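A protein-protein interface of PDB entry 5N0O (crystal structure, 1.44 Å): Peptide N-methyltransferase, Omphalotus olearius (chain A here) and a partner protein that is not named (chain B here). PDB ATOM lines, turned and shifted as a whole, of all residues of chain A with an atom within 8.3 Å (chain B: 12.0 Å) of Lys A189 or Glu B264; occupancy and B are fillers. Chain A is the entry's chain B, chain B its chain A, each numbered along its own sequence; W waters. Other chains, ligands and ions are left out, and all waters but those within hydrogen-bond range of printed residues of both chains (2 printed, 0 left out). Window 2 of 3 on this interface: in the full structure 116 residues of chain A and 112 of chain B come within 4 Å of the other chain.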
ATOM      1  N   SER A 152       3.553  25.717   7.019  1.00  0.00           N
ATOM      2  CA  SER A 152       2.186  25.858   6.465  1.00  0.00           C
ATOM      3  C   SER A 152       1.165  26.295   7.526  1.00  0.00           C
ATOM      4  O   SER A 152       0.329  27.166   7.276  1.00  0.00           O
ATOM      5  CB  SER A 152       1.720  24.566   5.781  1.00  0.00           C
ATOM      6  OG  SER A 152       2.557  24.231   4.689  1.00  0.00           O
ATOM      7  N   LEU A 155       1.424  30.002   8.311  1.00  0.00           N
ATOM      8  CA  LEU A 155       0.696  30.809   7.318  1.00  0.00           C
ATOM      9  C   LEU A 155      -0.835  30.709   7.424  1.00  0.00           C
ATOM     10  O   LEU A 155      -1.524  31.743   7.483  1.00  0.00           O
ATOM     11  CB  LEU A 155       1.145  30.428   5.908  1.00  0.00           C
ATOM     12  CG  LEU A 155       2.614  30.702   5.580  1.00  0.00           C
ATOM     13  CD1 LEU A 155       2.960  30.102   4.226  1.00  0.00           C
ATOM     14  CD2 LEU A 155       2.927  32.192   5.622  1.00  0.00           C
ATOM     15  N   VAL A 172       9.718  24.069   5.559  1.00  0.00           N
ATOM     16  CA  VAL A 172       9.737  25.201   4.628  1.00  0.00           C
ATOM     17  C   VAL A 172       9.860  24.742   3.167  1.00  0.00           C
ATOM     18  O   VAL A 172       9.554  25.516   2.237  1.00  0.00           O
ATOM     19  CB  VAL A 172      10.844  26.233   4.984  1.00  0.00           C
ATOM     20  CG1 VAL A 172      10.565  26.892   6.335  1.00  0.00           C
ATOM     21  CG2 VAL A 172      12.250  25.626   4.966  1.00  0.00           C
ATOM     22  N   GLY A 173      10.296  23.496   2.956  1.00  0.00           N
ATOM     23  CA  GLY A 173      10.375  22.905   1.612  1.00  0.00           C
ATOM     24  C   GLY A 173       9.110  22.272   1.052  1.00  0.00           C
ATOM     25  O   GLY A 173       9.162  21.725  -0.054  1.00  0.00           O
ATOM     26  N   CSO A 174       7.980  22.330   1.766  1.00  0.00           N
ATOM     27  CA  CSO A 174       6.712  21.741   1.278  1.00  0.00           C
ATOM     28  CB  CSO A 174       6.577  20.278   1.729  1.00  0.00           C
ATOM     29  SG  CSO A 174       6.718  20.064   3.474  1.00  0.00           S
ATOM     30  C   CSO A 174       5.506  22.559   1.678  1.00  0.00           C
ATOM     31  O   CSO A 174       4.517  22.030   2.198  1.00  0.00           O
ATOM     32  OD  CSO A 174       8.414  19.704   3.531  1.00  0.00           O
ATOM     33  N   VAL A 175       5.558  23.858   1.386  1.00  0.00           N
ATOM     34  CA  VAL A 175       4.499  24.789   1.792  1.00  0.00           C
ATOM     35  C   VAL A 175       3.159  24.460   1.101  1.00  0.00           C
ATOM     36  O   VAL A 175       3.073  24.463  -0.127  1.00  0.00           O
ATOM     37  CB  VAL A 175       4.910  26.260   1.523  1.00  0.00           C
ATOM     38  CG1 VAL A 175       3.749  27.217   1.788  1.00  0.00           C
ATOM     39  CG2 VAL A 175       6.116  26.643   2.381  1.00  0.00           C
ATOM     40  N   GLY A 176       2.131  24.175   1.903  1.00  0.00           N
ATOM     41  CA  GLY A 176       0.778  23.877   1.407  1.00  0.00           C
ATOM     42  C   GLY A 176       0.569  22.535   0.717  1.00  0.00           C
ATOM     43  O   GLY A 176      -0.496  22.312   0.116  1.00  0.00           O
ATOM     44  N   ILE A 177       1.557  21.643   0.805  1.00  0.00           N
ATOM     45  CA  ILE A 177       1.558  20.363   0.087  1.00  0.00           C
ATOM     46  C   ILE A 177       1.118  19.243   1.038  1.00  0.00           C
ATOM     47  O   ILE A 177       1.696  19.082   2.114  1.00  0.00           O
ATOM     48  CB  ILE A 177       2.967  20.054  -0.482  1.00  0.00           C
ATOM     49  CG1 ILE A 177       3.369  21.118  -1.518  1.00  0.00           C
ATOM     50  CG2 ILE A 177       3.025  18.651  -1.094  1.00  0.00           C
ATOM     51  CD1 ILE A 177       4.803  21.016  -2.002  1.00  0.00           C
ATOM     52  N   ASP A 186       7.627  19.702  -5.408  1.00  0.00           N
ATOM     53  CA  ASP A 186       7.580  20.884  -6.271  1.00  0.00           C
ATOM     54  C   ASP A 186       7.048  22.042  -5.413  1.00  0.00           C
ATOM     55  O   ASP A 186       5.831  22.234  -5.288  1.00  0.00           O
ATOM     56  CB  ASP A 186       6.682  20.618  -7.489  1.00  0.00           C
ATOM     57  CG  ASP A 186       6.554  21.822  -8.421  1.00  0.00           C
ATOM     58  OD1 ASP A 186       7.341  22.790  -8.313  1.00  0.00           O
ATOM     59  OD2 ASP A 186       5.650  21.784  -9.281  1.00  0.00           O
ATOM     60  N   ASN A 187       7.972  22.811  -4.836  1.00  0.00           N
ATOM     61  CA  ASN A 187       7.661  23.784  -3.780  1.00  0.00           C
ATOM     62  C   ASN A 187       7.247  25.139  -4.377  1.00  0.00           C
ATOM     63  O   ASN A 187       7.861  26.172  -4.093  1.00  0.00           O
ATOM     64  CB  ASN A 187       8.888  23.915  -2.853  1.00  0.00           C
ATOM     65  CG  ASN A 187       8.564  24.551  -1.502  1.00  0.00           C
ATOM     66  OD1 ASN A 187       7.448  24.448  -0.988  1.00  0.00           O
ATOM     67  ND2 ASN A 187       9.561  25.200  -0.918  1.00  0.00           N
ATOM     68  N   ASN A 188       6.185  25.124  -5.187  1.00  0.00           N
ATOM     69  CA  ASN A 188       5.781  26.311  -5.967  1.00  0.00           C
ATOM     70  C   ASN A 188       4.912  27.327  -5.206  1.00  0.00           C
ATOM     71  O   ASN A 188       4.584  28.370  -5.767  1.00  0.00           O
ATOM     72  CB  ASN A 188       5.154  25.925  -7.335  1.00  0.00           C
ATOM     73  CG  ASN A 188       3.816  25.200  -7.226  1.00  0.00           C
ATOM     74  OD1 ASN A 188       3.149  25.205  -6.191  1.00  0.00           O
ATOM     75  ND2 ASN A 188       3.415  24.568  -8.326  1.00  0.00           N
ATOM     76  N   LYS A 189       4.564  27.041  -3.944  1.00  0.00           N
ATOM     77  CA  LYS A 189       3.900  28.020  -3.066  1.00  0.00           C
ATOM     78  C   LYS A 189       4.878  28.665  -2.061  1.00  0.00           C
ATOM     79  O   LYS A 189       4.451  29.397  -1.171  1.00  0.00           O
ATOM     80  CB  LYS A 189       2.723  27.371  -2.320  1.00  0.00           C
ATOM     81  CG  LYS A 189       1.645  26.770  -3.217  1.00  0.00           C
ATOM     82  CD  LYS A 189       0.825  27.847  -3.917  1.00  0.00           C
ATOM     83  CE  LYS A 189      -0.232  27.251  -4.837  1.00  0.00           C
ATOM     84  NZ  LYS A 189       0.358  26.494  -5.978  1.00  0.00           N
ATOM     85  N   PHE A 190       6.181  28.420  -2.231  1.00  0.00           N
ATOM     86  CA  PHE A 190       7.233  28.998  -1.372  1.00  0.00           C
ATOM     87  C   PHE A 190       7.220  30.538  -1.310  1.00  0.00           C
ATOM     88  O   PHE A 190       7.572  31.126  -0.285  1.00  0.00           O
ATOM     89  CB  PHE A 190       8.609  28.491  -1.844  1.00  0.00           C
ATOM     90  CG  PHE A 190       9.772  28.994  -1.027  1.00  0.00           C
ATOM     91  CD1 PHE A 190       9.977  28.554   0.276  1.00  0.00           C
ATOM     92  CD2 PHE A 190      10.673  29.906  -1.570  1.00  0.00           C
ATOM     93  CE1 PHE A 190      11.050  29.022   1.018  1.00  0.00           C
ATOM     94  CE2 PHE A 190      11.749  30.374  -0.834  1.00  0.00           C
ATOM     95  CZ  PHE A 190      11.940  29.926   0.465  1.00  0.00           C
ATOM     96  N   GLY A 191       6.798  31.189  -2.392  1.00  0.00           N
ATOM     97  CA  GLY A 191       6.692  32.644  -2.431  1.00  0.00           C
ATOM     98  C   GLY A 191       5.694  33.252  -1.457  1.00  0.00           C
ATOM     99  O   GLY A 191       5.840  34.417  -1.067  1.00  0.00           O
ATOM    100  N   VAL A 192       4.681  32.474  -1.073  1.00  0.00           N
ATOM    101  CA  VAL A 192       3.682  32.892  -0.089  1.00  0.00           C
ATOM    102  C   VAL A 192       4.347  33.025   1.297  1.00  0.00           C
ATOM    103  O   VAL A 192       4.034  33.954   2.056  1.00  0.00           O
ATOM    104  CB  VAL A 192       2.476  31.913  -0.019  1.00  0.00           C
ATOM    105  CG1 VAL A 192       1.458  32.377   1.021  1.00  0.00           C
ATOM    106  CG2 VAL A 192       1.801  31.763  -1.383  1.00  0.00           C
ATOM    107  N   LEU A 193       5.263  32.108   1.621  1.00  0.00           N
ATOM    108  CA  LEU A 193       6.069  32.216   2.855  1.00  0.00           C
ATOM    109  C   LEU A 193       7.004  33.433   2.826  1.00  0.00           C
ATOM    110  O   LEU A 193       7.104  34.170   3.812  1.00  0.00           O
ATOM    111  CB  LEU A 193       6.887  30.938   3.101  1.00  0.00           C
ATOM    112  CG  LEU A 193       7.838  30.947   4.310  1.00  0.00           C
ATOM    113  CD1 LEU A 193       7.088  31.185   5.615  1.00  0.00           C
ATOM    114  CD2 LEU A 193       8.621  29.643   4.365  1.00  0.00           C
ATOM    115  N   VAL A 194       7.658  33.660   1.686  1.00  0.00           N
ATOM    116  CA  VAL A 194       8.583  34.790   1.538  1.00  0.00           C
ATOM    117  C   VAL A 194       7.839  36.119   1.735  1.00  0.00           C
ATOM    118  O   VAL A 194       8.344  37.002   2.428  1.00  0.00           O
ATOM    119  CB  VAL A 194       9.343  34.775   0.181  1.00  0.00           C
ATOM    120  CG1 VAL A 194      10.243  36.000   0.043  1.00  0.00           C
ATOM    121  CG2 VAL A 194      10.175  33.499   0.037  1.00  0.00           C
ATOM    122  N   ASP A 195       6.647  36.250   1.140  1.00  0.00           N
ATOM    123  CA  ASP A 195       5.804  37.451   1.334  1.00  0.00           C
ATOM    124  C   ASP A 195       5.493  37.732   2.818  1.00  0.00           C
ATOM    125  O   ASP A 195       5.598  38.884   3.263  1.00  0.00           O
ATOM    126  CB  ASP A 195       4.483  37.355   0.534  1.00  0.00           C
ATOM    127  CG  ASP A 195       4.656  37.596  -0.977  1.00  0.00           C
ATOM    128  OD1 ASP A 195       5.725  38.054  -1.442  1.00  0.00           O
ATOM    129  OD2 ASP A 195       3.680  37.336  -1.719  1.00  0.00           O
ATOM    130  N   SER B 255      -8.662  29.836  10.740  1.00  0.00           N
ATOM    131  CA  SER B 255      -7.840  29.814   9.534  1.00  0.00           C
ATOM    132  C   SER B 255      -8.076  31.071   8.698  1.00  0.00           C
ATOM    133  O   SER B 255      -9.188  31.597   8.658  1.00  0.00           O
ATOM    134  CB  SER B 255      -8.133  28.563   8.710  1.00  0.00           C
ATOM    135  OG  SER B 255      -7.905  27.389   9.474  1.00  0.00           O
ATOM    136  N   ASN B 256      -7.021  31.542   8.038  1.00  0.00           N
ATOM    137  CA  ASN B 256      -7.082  32.732   7.190  1.00  0.00           C
ATOM    138  C   ASN B 256      -7.560  32.311   5.799  1.00  0.00           C
ATOM    139  O   ASN B 256      -6.912  31.497   5.140  1.00  0.00           O
ATOM    140  CB  ASN B 256      -5.699  33.391   7.121  1.00  0.00           C
ATOM    141  CG  ASN B 256      -5.705  34.698   6.350  1.00  0.00           C
ATOM    142  OD1 ASN B 256      -5.829  34.708   5.126  1.00  0.00           O
ATOM    143  ND2 ASN B 256      -5.544  35.810   7.062  1.00  0.00           N
ATOM    144  N   LEU B 257      -8.685  32.880   5.359  1.00  0.00           N
ATOM    145  CA  LEU B 257      -9.318  32.480   4.091  1.00  0.00           C
ATOM    146  C   LEU B 257      -8.515  32.884   2.850  1.00  0.00           C
ATOM    147  O   LEU B 257      -8.465  32.126   1.882  1.00  0.00           O
ATOM    148  CB  LEU B 257     -10.750  33.029   3.999  1.00  0.00           C
ATOM    149  CG  LEU B 257     -11.750  32.549   5.058  1.00  0.00           C
ATOM    150  CD1 LEU B 257     -13.118  33.160   4.787  1.00  0.00           C
ATOM    151  CD2 LEU B 257     -11.841  31.027   5.107  1.00  0.00           C
ATOM    152  N   ASP B 258      -7.883  34.058   2.886  1.00  0.00           N
ATOM    153  CA  ASP B 258      -7.003  34.503   1.795  1.00  0.00           C
ATOM    154  C   ASP B 258      -5.812  33.571   1.568  1.00  0.00           C
ATOM    155  O   ASP B 258      -5.461  33.286   0.427  1.00  0.00           O
ATOM    156  CB  ASP B 258      -6.497  35.934   2.033  1.00  0.00           C
ATOM    157  CG  ASP B 258      -7.602  36.971   1.949  1.00  0.00           C
ATOM    158  OD1 ASP B 258      -8.368  36.957   0.961  1.00  0.00           O
ATOM    159  OD2 ASP B 258      -7.703  37.809   2.871  1.00  0.00           O
ATOM    160  N   ILE B 259      -5.196  33.091   2.651  1.00  0.00           N
ATOM    161  CA  ILE B 259      -4.058  32.172   2.539  1.00  0.00           C
ATOM    162  C   ILE B 259      -4.501  30.818   1.968  1.00  0.00           C
ATOM    163  O   ILE B 259      -3.814  30.249   1.120  1.00  0.00           O
ATOM    164  CB  ILE B 259      -3.338  31.978   3.901  1.00  0.00           C
ATOM    165  CG1 ILE B 259      -2.708  33.298   4.383  1.00  0.00           C
ATOM    166  CG2 ILE B 259      -2.276  30.881   3.820  1.00  0.00           C
ATOM    167  CD1 ILE B 259      -1.446  33.719   3.654  1.00  0.00           C
ATOM    168  N   ILE B 260      -5.635  30.309   2.445  1.00  0.00           N
ATOM    169  CA  ILE B 260      -6.206  29.057   1.926  1.00  0.00           C
ATOM    170  C   ILE B 260      -6.496  29.162   0.415  1.00  0.00           C
ATOM    171  O   ILE B 260      -6.291  28.189  -0.315  1.00  0.00           O
ATOM    172  CB  ILE B 260      -7.459  28.619   2.738  1.00  0.00           C
ATOM    173  CG1 ILE B 260      -7.014  28.024   4.083  1.00  0.00           C
ATOM    174  CG2 ILE B 260      -8.299  27.592   1.977  1.00  0.00           C
ATOM    175  CD1 ILE B 260      -8.122  27.822   5.096  1.00  0.00           C
ATOM    176  N   ARG B 261      -6.948  30.333  -0.038  1.00  0.00           N
ATOM    177  CA  ARG B 261      -7.141  30.601  -1.472  1.00  0.00           C
ATOM    178  C   ARG B 261      -5.815  30.556  -2.241  1.00  0.00           C
ATOM    179  O   ARG B 261      -5.703  29.847  -3.243  1.00  0.00           O
ATOM    180  CB  ARG B 261      -7.827  31.957  -1.694  1.00  0.00           C
ATOM    181  CG  ARG B 261      -9.288  32.014  -1.271  1.00  0.00           C
ATOM    182  CD  ARG B 261      -9.743  33.452  -1.048  1.00  0.00           C
ATOM    183  NE  ARG B 261     -11.196  33.583  -0.919  1.00  0.00           N
ATOM    184  CZ  ARG B 261     -11.845  34.724  -0.663  1.00  0.00           C
ATOM    185  NH1 ARG B 261     -11.186  35.872  -0.499  1.00  0.00           N
ATOM    186  NH2 ARG B 261     -13.176  34.721  -0.571  1.00  0.00           N
ATOM    187  N   ARG B 262      -4.814  31.296  -1.756  1.00  0.00           N
ATOM    188  CA  ARG B 262      -3.489  31.351  -2.400  1.00  0.00           C
ATOM    189  C   ARG B 262      -2.741  30.012  -2.412  1.00  0.00           C
ATOM    190  O   ARG B 262      -1.972  29.747  -3.338  1.00  0.00           O
ATOM    191  CB  ARG B 262      -2.604  32.414  -1.740  1.00  0.00           C
ATOM    192  CG  ARG B 262      -3.070  33.843  -1.958  1.00  0.00           C
ATOM    193  CD  ARG B 262      -2.167  34.826  -1.233  1.00  0.00           C
ATOM    194  NE  ARG B 262      -0.828  34.880  -1.823  1.00  0.00           N
ATOM    195  CZ  ARG B 262       0.235  35.472  -1.270  1.00  0.00           C
ATOM    196  NH1 ARG B 262       0.152  36.082  -0.086  1.00  0.00           N
ATOM    197  NH2 ARG B 262       1.403  35.452  -1.911  1.00  0.00           N
ATOM    198  N   LEU B 263      -2.941  29.196  -1.374  1.00  0.00           N
ATOM    199  CA  LEU B 263      -2.404  27.829  -1.333  1.00  0.00           C
ATOM    200  C   LEU B 263      -3.317  26.806  -2.034  1.00  0.00           C
ATOM    201  O   LEU B 263      -2.866  25.702  -2.346  1.00  0.00           O
ATOM    202  CB  LEU B 263      -2.153  27.389   0.115  1.00  0.00           C
ATOM    203  CG  LEU B 263      -1.136  28.197   0.933  1.00  0.00           C
ATOM    204  CD1 LEU B 263      -1.137  27.716   2.375  1.00  0.00           C
ATOM    205  CD2 LEU B 263       0.264  28.113   0.342  1.00  0.00           C
ATOM    206  N   GLU B 264      -4.589  27.168  -2.240  1.00  0.00           N
ATOM    207  CA  GLU B 264      -5.557  26.401  -3.048  1.00  0.00           C
ATOM    208  C   GLU B 264      -5.966  25.097  -2.350  1.00  0.00           C
ATOM    209  O   GLU B 264      -5.581  24.000  -2.773  1.00  0.00           O
ATOM    210  CB  GLU B 264      -5.033  26.147  -4.478  1.00  0.00           C
ATOM    211  CG  GLU B 264      -4.607  27.412  -5.222  1.00  0.00           C
ATOM    212  CD  GLU B 264      -3.953  27.137  -6.570  1.00  0.00           C
ATOM    213  OE1 GLU B 264      -4.265  27.862  -7.538  1.00  0.00           O
ATOM    214  OE2 GLU B 264      -3.118  26.211  -6.668  1.00  0.00           O
ATOM    215  N   LEU B 265      -6.745  25.243  -1.274  1.00  0.00           N
ATOM    216  CA  LEU B 265      -7.165  24.116  -0.418  1.00  0.00           C
ATOM    217  C   LEU B 265      -8.676  24.009  -0.096  1.00  0.00           C
ATOM    218  O   LEU B 265      -9.084  23.048   0.563  1.00  0.00           O
ATOM    219  CB  LEU B 265      -6.372  24.157   0.897  1.00  0.00           C
ATOM    220  CG  LEU B 265      -4.843  24.117   0.798  1.00  0.00           C
ATOM    221  CD1 LEU B 265      -4.212  24.473   2.134  1.00  0.00           C
ATOM    222  CD2 LEU B 265      -4.364  22.753   0.321  1.00  0.00           C
ATOM    223  N   LEU B 266      -9.501  24.958  -0.553  1.00  0.00           N
ATOM    224  CA  LEU B 266     -10.950  24.932  -0.256  1.00  0.00           C
ATOM    225  C   LEU B 266     -11.668  23.844  -1.057  1.00  0.00           C
ATOM    226  O   LEU B 266     -11.820  23.952  -2.274  1.00  0.00           O
ATOM    227  CB  LEU B 266     -11.611  26.300  -0.512  1.00  0.00           C
ATOM    228  CG  LEU B 266     -11.737  27.225   0.706  1.00  0.00           C
ATOM    229  CD1 LEU B 266     -11.924  28.675   0.278  1.00  0.00           C
ATOM    230  CD2 LEU B 266     -12.871  26.784   1.626  1.00  0.00           C
ATOM    231  N   PRO B 272     -13.748  25.975   6.655  1.00  0.00           N
ATOM    232  CA  PRO B 272     -12.922  25.322   7.673  1.00  0.00           C
ATOM    233  C   PRO B 272     -13.459  25.510   9.096  1.00  0.00           C
ATOM    234  O   PRO B 272     -13.534  26.641   9.584  1.00  0.00           O
ATOM    235  CB  PRO B 272     -11.561  26.008   7.511  1.00  0.00           C
ATOM    236  CG  PRO B 272     -11.886  27.366   6.999  1.00  0.00           C
ATOM    237  CD  PRO B 272     -13.133  27.228   6.171  1.00  0.00           C
HETATM  238  O   HOH W   1       1.901  35.652   2.313  1.00  0.00           O
HETATM  239  O   HOH W   2      -0.643  23.629  -2.769  1.00  0.00           O
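Printed residues of chain B within 4 Å of Leu A155: Ile B259 (3.7 Å). Of chain B, only Leu B263 (3.9 Å) comes within 4 Å of Val A175. No residue of chain B comes within 4 Å of Asn A187. Lys A189 touches three residues of chain B. No residue of chain B comes within 4 Å of Phe A190. Of chain B, only Arg B262 comes within 4 Å of Val A192. No residue of chain B comes within 4 Å of Leu A193. Printed residues of chain B within 4 Å of Asp A195: Arg B262 (3.0 Å). Printed residues of chain A within 4 Å of Leu B263: Val A175 and Lys A189. Of chain A, only Lys A189 (3.6 Å) comes within 4 Å of Glu B264. Of the printed residues of chain A, Leu B265 touches Gly A176 (3.9 Å). The nearest residue of chain A that does not touch Glu B264 is Gly A176 (6.1 Å).
Of the 18 printed residues of chain A, 6 touch a printed residue of chain B. Printed residues of chain A that touch a printed residue of chain B: Leu A155, Val A175, Gly A176, Lys A189, Val A192 and Asp A195. Hydrophobic or aromatic side chains of chain A within 4 Å of the printed part of chain B: Val A175 and Val A192. Hydrophobic or aromatic side chains of chain B within 4 Å of the printed part of chain A: Ile B259, Leu B263 and Leu B265. Among the printed residues, Asp or Glu carboxylates within 4 Å of a Lys or Arg side-chain nitrogen of the other chain: Lys A189 with Glu B264 and Asp A195 with Arg B262.
Water W1 lies within hydrogen-bond range of O of Val A192 (2.7 Å) and NH1 of Arg B262 (3.0 Å). Water W2 bridges the backbone carbonyl oxygen of Leu B263 (3.1 Å) and the backbone carbonyl oxygen of Gly A176 (3.2 Å).
OD1 of Asn B256 is in hydrogen-bond range of N of Ile B259, 3.0 Å away. The backbone NH (N) of Leu B265 lies within hydrogen-bond range of the backbone carbonyl oxygen (O) of Ile B260. The backbone NH (N) of Gly A176 sits at hydrogen-bond distance from the side-chain hydroxyl (OG) of Ser A152, 2.8 Å away. The backbone NH (N) of Val A175 lies within hydrogen-bond range of the side-chain amide oxygen (OD1) of Asn A187 (3.1 Å). The side-chain amide oxygen (OD1) of Asn A188 sits at hydrogen-bond distance from the side-chain amino group (NZ) of Lys A189 (3.1 Å).
NH2 of Arg B262 lies within salt-bridge range of OD2 of Asp A195 (3.0 Å). The side-chain carboxylate (OE2) of Glu B264 lies within salt-bridge range of the side-chain amino group (NZ) of Lys A189 (3.6 Å).
Among the printed residues, merely in contact across the chains: Leu A155 with Ile B259 (3.7 Å), Val A175 with Leu B263 (3.9 Å), Gly A176 with Leu B265 (3.9 Å), Lys A189 with Arg B262 (3.4 Å), Lys A189 with Leu B263 (3.7 Å) and Val A192 with Arg B262 (3.7 Å).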
